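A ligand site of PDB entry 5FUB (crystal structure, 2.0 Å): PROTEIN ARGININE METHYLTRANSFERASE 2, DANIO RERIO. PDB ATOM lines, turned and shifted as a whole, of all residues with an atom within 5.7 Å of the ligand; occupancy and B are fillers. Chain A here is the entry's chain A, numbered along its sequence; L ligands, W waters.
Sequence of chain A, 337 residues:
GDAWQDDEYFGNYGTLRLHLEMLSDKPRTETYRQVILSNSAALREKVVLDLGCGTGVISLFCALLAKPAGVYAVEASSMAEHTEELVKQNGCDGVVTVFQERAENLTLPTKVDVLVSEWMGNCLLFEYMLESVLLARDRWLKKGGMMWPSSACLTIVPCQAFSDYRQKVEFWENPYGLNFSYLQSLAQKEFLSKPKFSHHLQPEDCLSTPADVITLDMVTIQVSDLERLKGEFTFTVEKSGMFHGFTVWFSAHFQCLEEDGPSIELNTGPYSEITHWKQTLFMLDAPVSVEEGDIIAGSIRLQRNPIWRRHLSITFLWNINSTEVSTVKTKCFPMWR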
ATOM      1  N   TYR A   9     -19.035  37.364 -17.007  1.00  0.00           N
ATOM      2  CA  TYR A   9     -18.166  36.206 -16.776  1.00  0.00           C
ATOM      3  C   TYR A   9     -18.587  35.430 -15.532  1.00  0.00           C
ATOM      4  O   TYR A   9     -18.823  34.227 -15.585  1.00  0.00           O
ATOM      5  CB  TYR A   9     -16.704  36.663 -16.652  1.00  0.00           C
ATOM      6  CG  TYR A   9     -15.727  35.558 -16.326  1.00  0.00           C
ATOM      7  CD1 TYR A   9     -15.215  34.751 -17.331  1.00  0.00           C
ATOM      8  CD2 TYR A   9     -15.300  35.342 -15.022  1.00  0.00           C
ATOM      9  CE1 TYR A   9     -14.306  33.740 -17.041  1.00  0.00           C
ATOM     10  CE2 TYR A   9     -14.398  34.324 -14.722  1.00  0.00           C
ATOM     11  CZ  TYR A   9     -13.901  33.537 -15.740  1.00  0.00           C
ATOM     12  OH  TYR A   9     -13.014  32.538 -15.453  1.00  0.00           O
ATOM     13  N   PHE A  10     -18.679  36.118 -14.381  1.00  0.00           N
ATOM     14  CA  PHE A  10     -19.058  35.414 -13.165  1.00  0.00           C
ATOM     15  C   PHE A  10     -20.546  35.096 -13.136  1.00  0.00           C
ATOM     16  O   PHE A  10     -20.943  34.123 -12.489  1.00  0.00           O
ATOM     17  CB  PHE A  10     -18.664  36.221 -11.931  1.00  0.00           C
ATOM     18  CG  PHE A  10     -17.168  36.326 -11.745  1.00  0.00           C
ATOM     19  CD1 PHE A  10     -16.416  35.203 -11.448  1.00  0.00           C
ATOM     20  CD2 PHE A  10     -16.526  37.544 -11.876  1.00  0.00           C
ATOM     21  CE1 PHE A  10     -15.051  35.292 -11.273  1.00  0.00           C
ATOM     22  CE2 PHE A  10     -15.154  37.651 -11.713  1.00  0.00           C
ATOM     23  CZ  PHE A  10     -14.423  36.512 -11.401  1.00  0.00           C
ATOM     24  N   TYR A  13     -20.840  31.691 -14.626  1.00  0.00           N
ATOM     25  CA  TYR A  13     -20.419  30.630 -13.722  1.00  0.00           C
ATOM     26  C   TYR A  13     -21.306  30.487 -12.495  1.00  0.00           C
ATOM     27  O   TYR A  13     -21.056  29.597 -11.667  1.00  0.00           O
ATOM     28  CB  TYR A  13     -18.964  30.859 -13.295  1.00  0.00           C
ATOM     29  CG  TYR A  13     -17.963  30.386 -14.333  1.00  0.00           C
ATOM     30  CD1 TYR A  13     -17.854  29.032 -14.638  1.00  0.00           C
ATOM     31  CD2 TYR A  13     -17.139  31.284 -15.004  1.00  0.00           C
ATOM     32  CE1 TYR A  13     -16.950  28.584 -15.584  1.00  0.00           C
ATOM     33  CE2 TYR A  13     -16.235  30.837 -15.951  1.00  0.00           C
ATOM     34  CZ  TYR A  13     -16.141  29.489 -16.230  1.00  0.00           C
ATOM     35  OH  TYR A  13     -15.252  29.033 -17.171  1.00  0.00           O
ATOM     36  N   HIS A  19     -20.955  24.453 -15.201  1.00  0.00           N
ATOM     37  CA  HIS A  19     -20.397  23.458 -14.293  1.00  0.00           C
ATOM     38  C   HIS A  19     -20.750  22.045 -14.740  1.00  0.00           C
ATOM     39  O   HIS A  19     -19.941  21.125 -14.595  1.00  0.00           O
ATOM     40  CB  HIS A  19     -20.854  23.722 -12.868  1.00  0.00           C
ATOM     41  CG  HIS A  19     -20.349  25.012 -12.310  1.00  0.00           C
ATOM     42  ND1 HIS A  19     -19.037  25.207 -11.955  1.00  0.00           N
ATOM     43  CD2 HIS A  19     -20.976  26.190 -12.094  1.00  0.00           C
ATOM     44  CE1 HIS A  19     -18.877  26.447 -11.521  1.00  0.00           C
ATOM     45  NE2 HIS A  19     -20.036  27.062 -11.595  1.00  0.00           N
ATOM     46  N   MET A  22     -18.167  21.239 -17.304  1.00  0.00           N
ATOM     47  CA  MET A  22     -16.861  20.888 -16.726  1.00  0.00           C
ATOM     48  C   MET A  22     -16.892  19.515 -16.078  1.00  0.00           C
ATOM     49  O   MET A  22     -15.983  18.705 -16.264  1.00  0.00           O
ATOM     50  CB  MET A  22     -16.435  21.951 -15.718  1.00  0.00           C
ATOM     51  CG  MET A  22     -16.603  23.364 -16.196  1.00  0.00           C
ATOM     52  SD  MET A  22     -15.145  24.380 -15.952  1.00  0.00           S
ATOM     53  CE  MET A  22     -14.053  23.655 -17.164  1.00  0.00           C
ATOM     54  N   LEU A  23     -17.943  19.231 -15.297  1.00  0.00           N
ATOM     55  CA  LEU A  23     -17.994  17.974 -14.568  1.00  0.00           C
ATOM     56  C   LEU A  23     -18.302  16.799 -15.485  1.00  0.00           C
ATOM     57  O   LEU A  23     -17.903  15.665 -15.197  1.00  0.00           O
ATOM     58  CB  LEU A  23     -19.012  18.056 -13.440  1.00  0.00           C
ATOM     59  CG  LEU A  23     -18.646  19.095 -12.367  1.00  0.00           C
ATOM     60  CD1 LEU A  23     -19.721  19.204 -11.301  1.00  0.00           C
ATOM     61  CD2 LEU A  23     -17.295  18.766 -11.746  1.00  0.00           C
ATOM     62  N   ARG A  28     -10.933  15.777 -18.141  1.00  0.00           N
ATOM     63  CA  ARG A  28     -10.541  16.943 -17.350  1.00  0.00           C
ATOM     64  C   ARG A  28     -10.666  16.660 -15.850  1.00  0.00           C
ATOM     65  O   ARG A  28      -9.705  16.825 -15.102  1.00  0.00           O
ATOM     66  CB  ARG A  28     -11.400  18.147 -17.737  1.00  0.00           C
ATOM     67  CG  ARG A  28     -11.059  19.431 -17.012  1.00  0.00           C
ATOM     68  CD  ARG A  28     -12.272  20.344 -16.914  1.00  0.00           C
ATOM     69  NE  ARG A  28     -13.191  19.878 -15.890  1.00  0.00           N
ATOM     70  CZ  ARG A  28     -13.262  20.382 -14.663  1.00  0.00           C
ATOM     71  NH1 ARG A  28     -12.469  21.390 -14.324  1.00  0.00           N
ATOM     72  NH2 ARG A  28     -14.125  19.898 -13.779  1.00  0.00           N
ATOM     73  N   ASP A  50      -7.595  26.097  -3.472  1.00  0.00           N
ATOM     74  CA  ASP A  50      -8.314  25.738  -4.696  1.00  0.00           C
ATOM     75  C   ASP A  50      -8.901  27.022  -5.275  1.00  0.00           C
ATOM     76  O   ASP A  50      -9.953  27.490  -4.836  1.00  0.00           O
ATOM     77  CB  ASP A  50      -9.392  24.697  -4.416  1.00  0.00           C
ATOM     78  CG  ASP A  50     -10.195  24.305  -5.657  1.00  0.00           C
ATOM     79  OD1 ASP A  50      -9.837  24.729  -6.788  1.00  0.00           O
ATOM     80  OD2 ASP A  50     -11.186  23.559  -5.511  1.00  0.00           O
ATOM     81  N   LEU A  51      -8.217  27.583  -6.265  1.00  0.00           N
ATOM     82  CA  LEU A  51      -8.537  28.919  -6.764  1.00  0.00           C
ATOM     83  C   LEU A  51      -9.566  28.798  -7.875  1.00  0.00           C
ATOM     84  O   LEU A  51      -9.272  28.298  -8.966  1.00  0.00           O
ATOM     85  CB  LEU A  51      -7.281  29.621  -7.254  1.00  0.00           C
ATOM     86  CG  LEU A  51      -7.482  31.103  -7.508  1.00  0.00           C
ATOM     87  CD1 LEU A  51      -7.915  31.802  -6.224  1.00  0.00           C
ATOM     88  CD2 LEU A  51      -6.202  31.699  -8.008  1.00  0.00           C
ATOM     89  N   GLY A  52     -10.780  29.288  -7.615  1.00  0.00           N
ATOM     90  CA  GLY A  52     -11.863  29.167  -8.570  1.00  0.00           C
ATOM     91  C   GLY A  52     -12.461  27.781  -8.505  1.00  0.00           C
ATOM     92  O   GLY A  52     -12.452  27.036  -9.492  1.00  0.00           O
ATOM     93  N   CYS A  53     -12.990  27.414  -7.331  1.00  0.00           N
ATOM     94  CA  CYS A  53     -13.382  26.049  -7.039  1.00  0.00           C
ATOM     95  C   CYS A  53     -14.718  25.652  -7.666  1.00  0.00           C
ATOM     96  O   CYS A  53     -15.019  24.449  -7.708  1.00  0.00           O
ATOM     97  CB  CYS A  53     -13.447  25.833  -5.520  1.00  0.00           C
ATOM     98  SG  CYS A  53     -14.739  26.763  -4.653  1.00  0.00           S
ATOM     99  N   GLY A  54     -15.506  26.601  -8.132  1.00  0.00           N
ATOM    100  CA  GLY A  54     -16.787  26.264  -8.730  1.00  0.00           C
ATOM    101  C   GLY A  54     -17.678  25.546  -7.728  1.00  0.00           C
ATOM    102  O   GLY A  54     -17.941  26.043  -6.631  1.00  0.00           O
ATOM    103  N   THR A  55     -18.118  24.340  -8.093  1.00  0.00           N
ATOM    104  CA  THR A  55     -18.895  23.491  -7.197  1.00  0.00           C
ATOM    105  C   THR A  55     -18.068  22.952  -6.029  1.00  0.00           C
ATOM    106  O   THR A  55     -18.637  22.379  -5.100  1.00  0.00           O
ATOM    107  CB  THR A  55     -19.503  22.305  -7.953  1.00  0.00           C
ATOM    108  OG1 THR A  55     -18.467  21.545  -8.581  1.00  0.00           O
ATOM    109  CG2 THR A  55     -20.486  22.798  -9.011  1.00  0.00           C
ATOM    110  N   GLY A  56     -16.749  23.124  -6.073  1.00  0.00           N
ATOM    111  CA  GLY A  56     -15.878  22.634  -5.020  1.00  0.00           C
ATOM    112  C   GLY A  56     -15.308  21.257  -5.248  1.00  0.00           C
ATOM    113  O   GLY A  56     -14.727  20.690  -4.317  1.00  0.00           O
ATOM    114  N   VAL A  57     -15.424  20.725  -6.469  1.00  0.00           N
ATOM    115  CA  VAL A  57     -15.090  19.321  -6.729  1.00  0.00           C
ATOM    116  C   VAL A  57     -13.620  19.042  -6.414  1.00  0.00           C
ATOM    117  O   VAL A  57     -13.291  18.033  -5.772  1.00  0.00           O
ATOM    118  CB  VAL A  57     -15.440  18.955  -8.176  1.00  0.00           C
ATOM    119  CG1 VAL A  57     -14.928  20.019  -9.141  1.00  0.00           C
ATOM    120  CG2 VAL A  57     -14.875  17.589  -8.537  1.00  0.00           C
ATOM    121  N   ILE A  58     -12.718  19.929  -6.840  1.00  0.00           N
ATOM    122  CA  ILE A  58     -11.293  19.707  -6.586  1.00  0.00           C
ATOM    123  C   ILE A  58     -10.997  19.759  -5.100  1.00  0.00           C
ATOM    124  O   ILE A  58     -10.190  18.970  -4.577  1.00  0.00           O
ATOM    125  CB  ILE A  58     -10.436  20.727  -7.370  1.00  0.00           C
ATOM    126  CG1 ILE A  58     -10.701  20.617  -8.873  1.00  0.00           C
ATOM    127  CG2 ILE A  58      -8.952  20.524  -7.076  1.00  0.00           C
ATOM    128  CD1 ILE A  58      -9.960  21.665  -9.694  1.00  0.00           C
ATOM    129  N   VAL A  74     -11.997  28.848  -2.968  1.00  0.00           N
ATOM    130  CA  VAL A  74     -12.275  30.247  -3.293  1.00  0.00           C
ATOM    131  C   VAL A  74     -13.079  30.305  -4.587  1.00  0.00           C
ATOM    132  O   VAL A  74     -12.658  29.731  -5.602  1.00  0.00           O
ATOM    133  CB  VAL A  74     -10.963  31.051  -3.412  1.00  0.00           C
ATOM    134  CG1 VAL A  74     -11.243  32.453  -3.915  1.00  0.00           C
ATOM    135  CG2 VAL A  74     -10.243  31.112  -2.064  1.00  0.00           C
ATOM    136  N   GLU A  75     -14.219  30.986  -4.549  1.00  0.00           N
ATOM    137  CA  GLU A  75     -15.079  31.101  -5.723  1.00  0.00           C
ATOM    138  C   GLU A  75     -15.794  32.444  -5.687  1.00  0.00           C
ATOM    139  O   GLU A  75     -16.481  32.759  -4.705  1.00  0.00           O
ATOM    140  CB  GLU A  75     -16.094  29.949  -5.781  1.00  0.00           C
ATOM    141  CG  GLU A  75     -17.181  30.163  -6.813  1.00  0.00           C
ATOM    142  CD  GLU A  75     -16.620  30.204  -8.223  1.00  0.00           C
ATOM    143  OE1 GLU A  75     -15.759  29.369  -8.548  1.00  0.00           O
ATOM    144  OE2 GLU A  75     -17.045  31.081  -9.007  1.00  0.00           O
ATOM    145  N   ALA A  76     -15.667  33.231  -6.759  1.00  0.00           N
ATOM    146  CA  ALA A  76     -16.216  34.588  -6.772  1.00  0.00           C
ATOM    147  C   ALA A  76     -17.671  34.640  -7.227  1.00  0.00           C
ATOM    148  O   ALA A  76     -18.344  35.641  -6.939  1.00  0.00           O
ATOM    149  CB  ALA A  76     -15.378  35.488  -7.692  1.00  0.00           C
ATOM    150  N   SER A  77     -18.160  33.623  -7.919  1.00  0.00           N
ATOM    151  CA  SER A  77     -19.534  33.648  -8.415  1.00  0.00           C
ATOM    152  C   SER A  77     -20.505  33.241  -7.317  1.00  0.00           C
ATOM    153  O   SER A  77     -20.122  32.793  -6.232  1.00  0.00           O
ATOM    154  CB  SER A  77     -19.688  32.707  -9.613  1.00  0.00           C
ATOM    155  OG  SER A  77     -19.771  31.358  -9.175  1.00  0.00           O
ATOM    156  N   GLU A 101     -14.979  35.094  -2.685  1.00  0.00           N
ATOM    157  CA  GLU A 101     -14.126  36.249  -2.929  1.00  0.00           C
ATOM    158  C   GLU A 101     -13.447  36.082  -4.275  1.00  0.00           C
ATOM    159  O   GLU A 101     -13.278  34.966  -4.774  1.00  0.00           O
ATOM    160  CB  GLU A 101     -13.075  36.409  -1.814  1.00  0.00           C
ATOM    161  CG  GLU A 101     -13.671  36.612  -0.430  1.00  0.00           C
ATOM    162  CD  GLU A 101     -12.628  36.810   0.661  1.00  0.00           C
ATOM    163  OE1 GLU A 101     -11.444  37.036   0.330  1.00  0.00           O
ATOM    164  OE2 GLU A 101     -12.996  36.732   1.850  1.00  0.00           O
ATOM    165  N   ARG A 102     -13.075  37.220  -4.867  1.00  0.00           N
ATOM    166  CA  ARG A 102     -12.188  37.201  -6.023  1.00  0.00           C
ATOM    167  C   ARG A 102     -10.750  36.998  -5.568  1.00  0.00           C
ATOM    168  O   ARG A 102     -10.348  37.474  -4.490  1.00  0.00           O
ATOM    169  CB  ARG A 102     -12.292  38.495  -6.824  1.00  0.00           C
ATOM    170  CG  ARG A 102     -13.546  38.633  -7.687  1.00  0.00           C
ATOM    171  CD  ARG A 102     -13.337  39.748  -8.681  1.00  0.00           C
ATOM    172  NE  ARG A 102     -12.553  40.818  -8.081  1.00  0.00           N
ATOM    173  CZ  ARG A 102     -11.642  41.536  -8.733  1.00  0.00           C
ATOM    174  NH1 ARG A 102     -11.394  41.298 -10.013  1.00  0.00           N
ATOM    175  NH2 ARG A 102     -10.968  42.483  -8.085  1.00  0.00           N
ATOM    176  N   ALA A 103      -9.973  36.290  -6.388  1.00  0.00           N
ATOM    177  CA  ALA A 103      -8.559  36.107  -6.091  1.00  0.00           C
ATOM    178  C   ALA A 103      -7.843  37.437  -5.902  1.00  0.00           C
ATOM    179  O   ALA A 103      -6.926  37.536  -5.081  1.00  0.00           O
ATOM    180  CB  ALA A 103      -7.891  35.304  -7.208  1.00  0.00           C
ATOM    181  N   GLU A 104      -8.268  38.464  -6.637  1.00  0.00           N
ATOM    182  CA  GLU A 104      -7.598  39.759  -6.571  1.00  0.00           C
ATOM    183  C   GLU A 104      -7.818  40.451  -5.235  1.00  0.00           C
ATOM    184  O   GLU A 104      -6.930  41.163  -4.755  1.00  0.00           O
ATOM    185  CB  GLU A 104      -8.090  40.648  -7.722  1.00  0.00           C
ATOM    186  CG  GLU A 104      -7.678  40.159  -9.122  1.00  0.00           C
ATOM    187  CD  GLU A 104      -8.500  38.994  -9.641  1.00  0.00           C
ATOM    188  OE1 GLU A 104      -9.380  38.478  -8.911  1.00  0.00           O
ATOM    189  OE2 GLU A 104      -8.286  38.584 -10.809  1.00  0.00           O
ATOM    190  N   GLU A 118      -8.160  25.173 -11.983  1.00  0.00           N
ATOM    191  CA  GLU A 118      -8.495  24.827 -13.356  1.00  0.00           C
ATOM    192  C   GLU A 118      -8.795  26.151 -14.052  1.00  0.00           C
ATOM    193  O   GLU A 118      -9.946  26.608 -14.087  1.00  0.00           O
ATOM    194  CB  GLU A 118      -9.654  23.835 -13.414  1.00  0.00           C
ATOM    195  CG  GLU A 118      -9.674  23.010 -14.679  1.00  0.00           C
ATOM    196  CD  GLU A 118     -10.099  23.833 -15.871  1.00  0.00           C
ATOM    197  OE1 GLU A 118     -11.292  24.179 -15.940  1.00  0.00           O
ATOM    198  OE2 GLU A 118      -9.247  24.150 -16.724  1.00  0.00           O
ATOM    199  N   MET A 129      -8.012  33.932 -16.889  1.00  0.00           N
ATOM    200  CA  MET A 129      -8.077  33.567 -15.478  1.00  0.00           C
ATOM    201  C   MET A 129      -6.690  33.286 -14.917  1.00  0.00           C
ATOM    202  O   MET A 129      -6.478  33.407 -13.704  1.00  0.00           O
ATOM    203  CB  MET A 129      -8.996  32.349 -15.304  1.00  0.00           C
ATOM    204  CG  MET A 129      -9.087  31.837 -13.875  1.00  0.00           C
ATOM    205  SD  MET A 129     -10.237  30.454 -13.689  1.00  0.00           S
ATOM    206  CE  MET A 129      -9.856  29.943 -12.019  1.00  0.00           C
ATOM    207  N   SER A 132      -5.509  36.021 -12.594  1.00  0.00           N
ATOM    208  CA  SER A 132      -5.984  35.852 -11.223  1.00  0.00           C
ATOM    209  C   SER A 132      -5.164  34.811 -10.474  1.00  0.00           C
ATOM    210  O   SER A 132      -4.857  34.969  -9.285  1.00  0.00           O
ATOM    211  CB  SER A 132      -7.456  35.459 -11.204  1.00  0.00           C
ATOM    212  OG  SER A 132      -8.247  36.315 -12.013  1.00  0.00           O
ATOM    213  N   ARG A 310     -10.271  40.103 -21.020  1.00  0.00           N
ATOM    214  CA  ARG A 310     -10.454  38.659 -21.142  1.00  0.00           C
ATOM    215  C   ARG A 310     -10.261  38.172 -22.561  1.00  0.00           C
ATOM    216  O   ARG A 310     -10.343  36.961 -22.806  1.00  0.00           O
ATOM    217  CB  ARG A 310     -11.837  38.253 -20.614  1.00  0.00           C
ATOM    218  CG  ARG A 310     -11.966  38.472 -19.099  1.00  0.00           C
ATOM    219  CD  ARG A 310     -13.036  37.595 -18.478  1.00  0.00           C
ATOM    220  NE  ARG A 310     -13.174  37.894 -17.045  1.00  0.00           N
ATOM    221  CZ  ARG A 310     -12.510  37.282 -16.081  1.00  0.00           C
ATOM    222  NH1 ARG A 310     -11.633  36.330 -16.359  1.00  0.00           N
ATOM    223  NH2 ARG A 310     -12.723  37.625 -14.817  1.00  0.00           N
HETATM  224  N1  LIG L   1     -12.740  24.231 -10.130  1.00  0.00           N
HETATM  225  C1  LIG L   1     -14.015  23.956 -10.715  1.00  0.00           C
HETATM  226  C2  LIG L   1     -14.453  25.059 -11.626  1.00  0.00           C
HETATM  227  C3  LIG L   1     -13.552  25.442 -12.805  1.00  0.00           C
HETATM  228  S1  LIG L   1     -14.064  26.803 -13.815  1.00  0.00           S
HETATM  229  C4  LIG L   1     -13.933  22.671 -11.517  1.00  0.00           C
HETATM  230  O1  LIG L   1     -12.806  22.225 -11.884  1.00  0.00           O
HETATM  231  O2  LIG L   1     -14.993  22.048 -11.811  1.00  0.00           O
HETATM  232  C5  LIG L   1     -13.425  28.361 -13.135  1.00  0.00           C
HETATM  233  C6  LIG L   1     -14.027  28.850 -11.887  1.00  0.00           C
HETATM  234  O3  LIG L   1     -13.148  29.771 -11.318  1.00  0.00           O
HETATM  235  C7  LIG L   1     -15.310  29.557 -12.122  1.00  0.00           C
HETATM  236  O4  LIG L   1     -16.275  29.115 -11.176  1.00  0.00           O
HETATM  237  C8  LIG L   1     -15.023  30.919 -11.924  1.00  0.00           C
HETATM  238  O5  LIG L   1     -16.125  31.628 -11.345  1.00  0.00           O
HETATM  239  C9  LIG L   1     -13.883  30.899 -10.976  1.00  0.00           C
HETATM  240  N2  LIG L   1     -13.041  32.081 -11.057  1.00  0.00           N
HETATM  241  C10 LIG L   1     -12.503  32.597 -12.177  1.00  0.00           C
HETATM  242  N3  LIG L   1     -11.788  33.675 -11.839  1.00  0.00           N
HETATM  243  C11 LIG L   1     -11.867  33.842 -10.496  1.00  0.00           C
HETATM  244  C12 LIG L   1     -11.334  34.780  -9.621  1.00  0.00           C
HETATM  245  N4  LIG L   1     -10.509  35.839 -10.105  1.00  0.00           N
HETATM  246  N5  LIG L   1     -11.601  34.658  -8.308  1.00  0.00           N
HETATM  247  C13 LIG L   1     -12.377  33.670  -7.847  1.00  0.00           C
HETATM  248  N6  LIG L   1     -12.916  32.751  -8.670  1.00  0.00           N
HETATM  249  C14 LIG L   1     -12.668  32.812  -9.993  1.00  0.00           C
HETATM  250  O   HOH W   1     -10.082  25.470 -10.022  1.00  0.00           O
HETATM  251  O   HOH W   2     -13.086  22.662  -7.501  1.00  0.00           O
HETATM  252  O   HOH W   3     -10.708  35.641 -13.712  1.00  0.00           O
HETATM  253  O   HOH W   4     -17.492  23.074 -10.720  1.00  0.00           O
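The backbone carbonyl oxygen (O) of Gly 52 sits at hydrogen-bond distance from a nitrogen (N1) of the ligand, 2.9 Å away.
The side-chain carboxylate (OE1) of Glu 104 sits at hydrogen-bond distance from a nitrogen (N4) of the ligand, at 3.1 Å.
The side-chain hydroxyl of Ser 132 lies within hydrogen-bond range of a nitrogen (N4) of the ligand, 3.0 Å away.
O of Cys 53 sits close to N1 of the ligand, 3.3 Å away.
N of Ala 103 sits at hydrogen-bond distance from N5 of the ligand (3.0 Å).
The guanidinium group (NH1) of Arg 28 is in salt-bridge range of an oxygen (O1) of the ligand, 2.6 Å away.
A nitrogen (N6) of the ligand lies within hydrogen-bond range of the backbone NH of Ala 76.
O5 of the ligand sits at hydrogen-bond distance from OE2 of Glu 75 (2.6 Å).
The guanidinium group (NE) of Arg 28 lies within hydrogen-bond range of the backbone carbonyl oxygen (O) of Met 22.
The backbone carbonyl oxygen (O) of Tyr 13 sits at hydrogen-bond distance from a ring nitrogen (NE2) of His 19, 2.7 Å away.
The backbone carbonyl oxygen (O) of Glu 75 is in hydrogen-bond range of the backbone NH (N) of Glu 101 (3.4 Å).
NH1 of Arg 102 is in salt-bridge range of OE1 of Glu 104 (3.6 Å).
N of Cys 53 lies within hydrogen-bond range of O of Val 74 (2.9 Å).
The guanidinium group (NH1) of Arg 28 is in salt-bridge range of the side-chain carboxylate (OE1) of Glu 118, at 3.4 Å.
O of Tyr 13 sits at hydrogen-bond distance from OG of Ser 77 (3.3 Å).
The backbone carbonyl oxygen of Val 74 lies within hydrogen-bond range of the backbone NH of Gly 52, 2.8 Å away.
A sulfur (S1) of the ligand sits close to the side-chain sulfur of Met 22, 3.4 Å away.
Residues that only touch the ligand: Tyr 9 (3.3 Å), Phe 10 (3.6 Å), Tyr 13 (3.5 Å), His 19 (3.7 Å), Gly 54 (3.8 Å), Val 57 (3.4 Å), Ile 58 (3.6 Å), Glu 101 (3.5 Å), Arg 102 (3.5 Å), Glu 118 (3.9 Å) and Met 129 (3.4 Å).
Hydrophobic or aromatic side chains within 4 Å of the ligand: Tyr 9, Phe 10, Tyr 13, His 19, Met 22, Val 57, Ile 58, Ala 76, Ala 103 and Met 129.
20 residues have an atom within 4 Å of the ligand: Tyr 9, Phe 10, Tyr 13, His 19, Met 22, Arg 28, Gly 52, Cys 53, Gly 54, Val 57, Ile 58, Glu 75, Ala 76, Glu 101, Arg 102, Ala 103, Glu 104, Glu 118, Met 129 and Ser 132.
Water W4 lies within hydrogen-bond range of OG1 of Thr 55 (2.8 Å), ND1 of His 19 (2.9 Å) and O2 of the ligand (2.9 Å).
Water W3 lies within hydrogen-bond range of the guanidinium group of Arg 310, a nitrogen (N3) of the ligand and the side-chain hydroxyl of Ser 132.
Water W2 lies within hydrogen-bond range of the backbone carbonyl oxygen of Cys 53 (2.6 Å), the backbone NH of Ile 58 (2.8 Å), the side-chain carboxylate of Asp 50 (2.9 Å), a nitrogen (N1) of the ligand (3.1 Å) and the backbone NH of Val 57 (3.2 Å).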
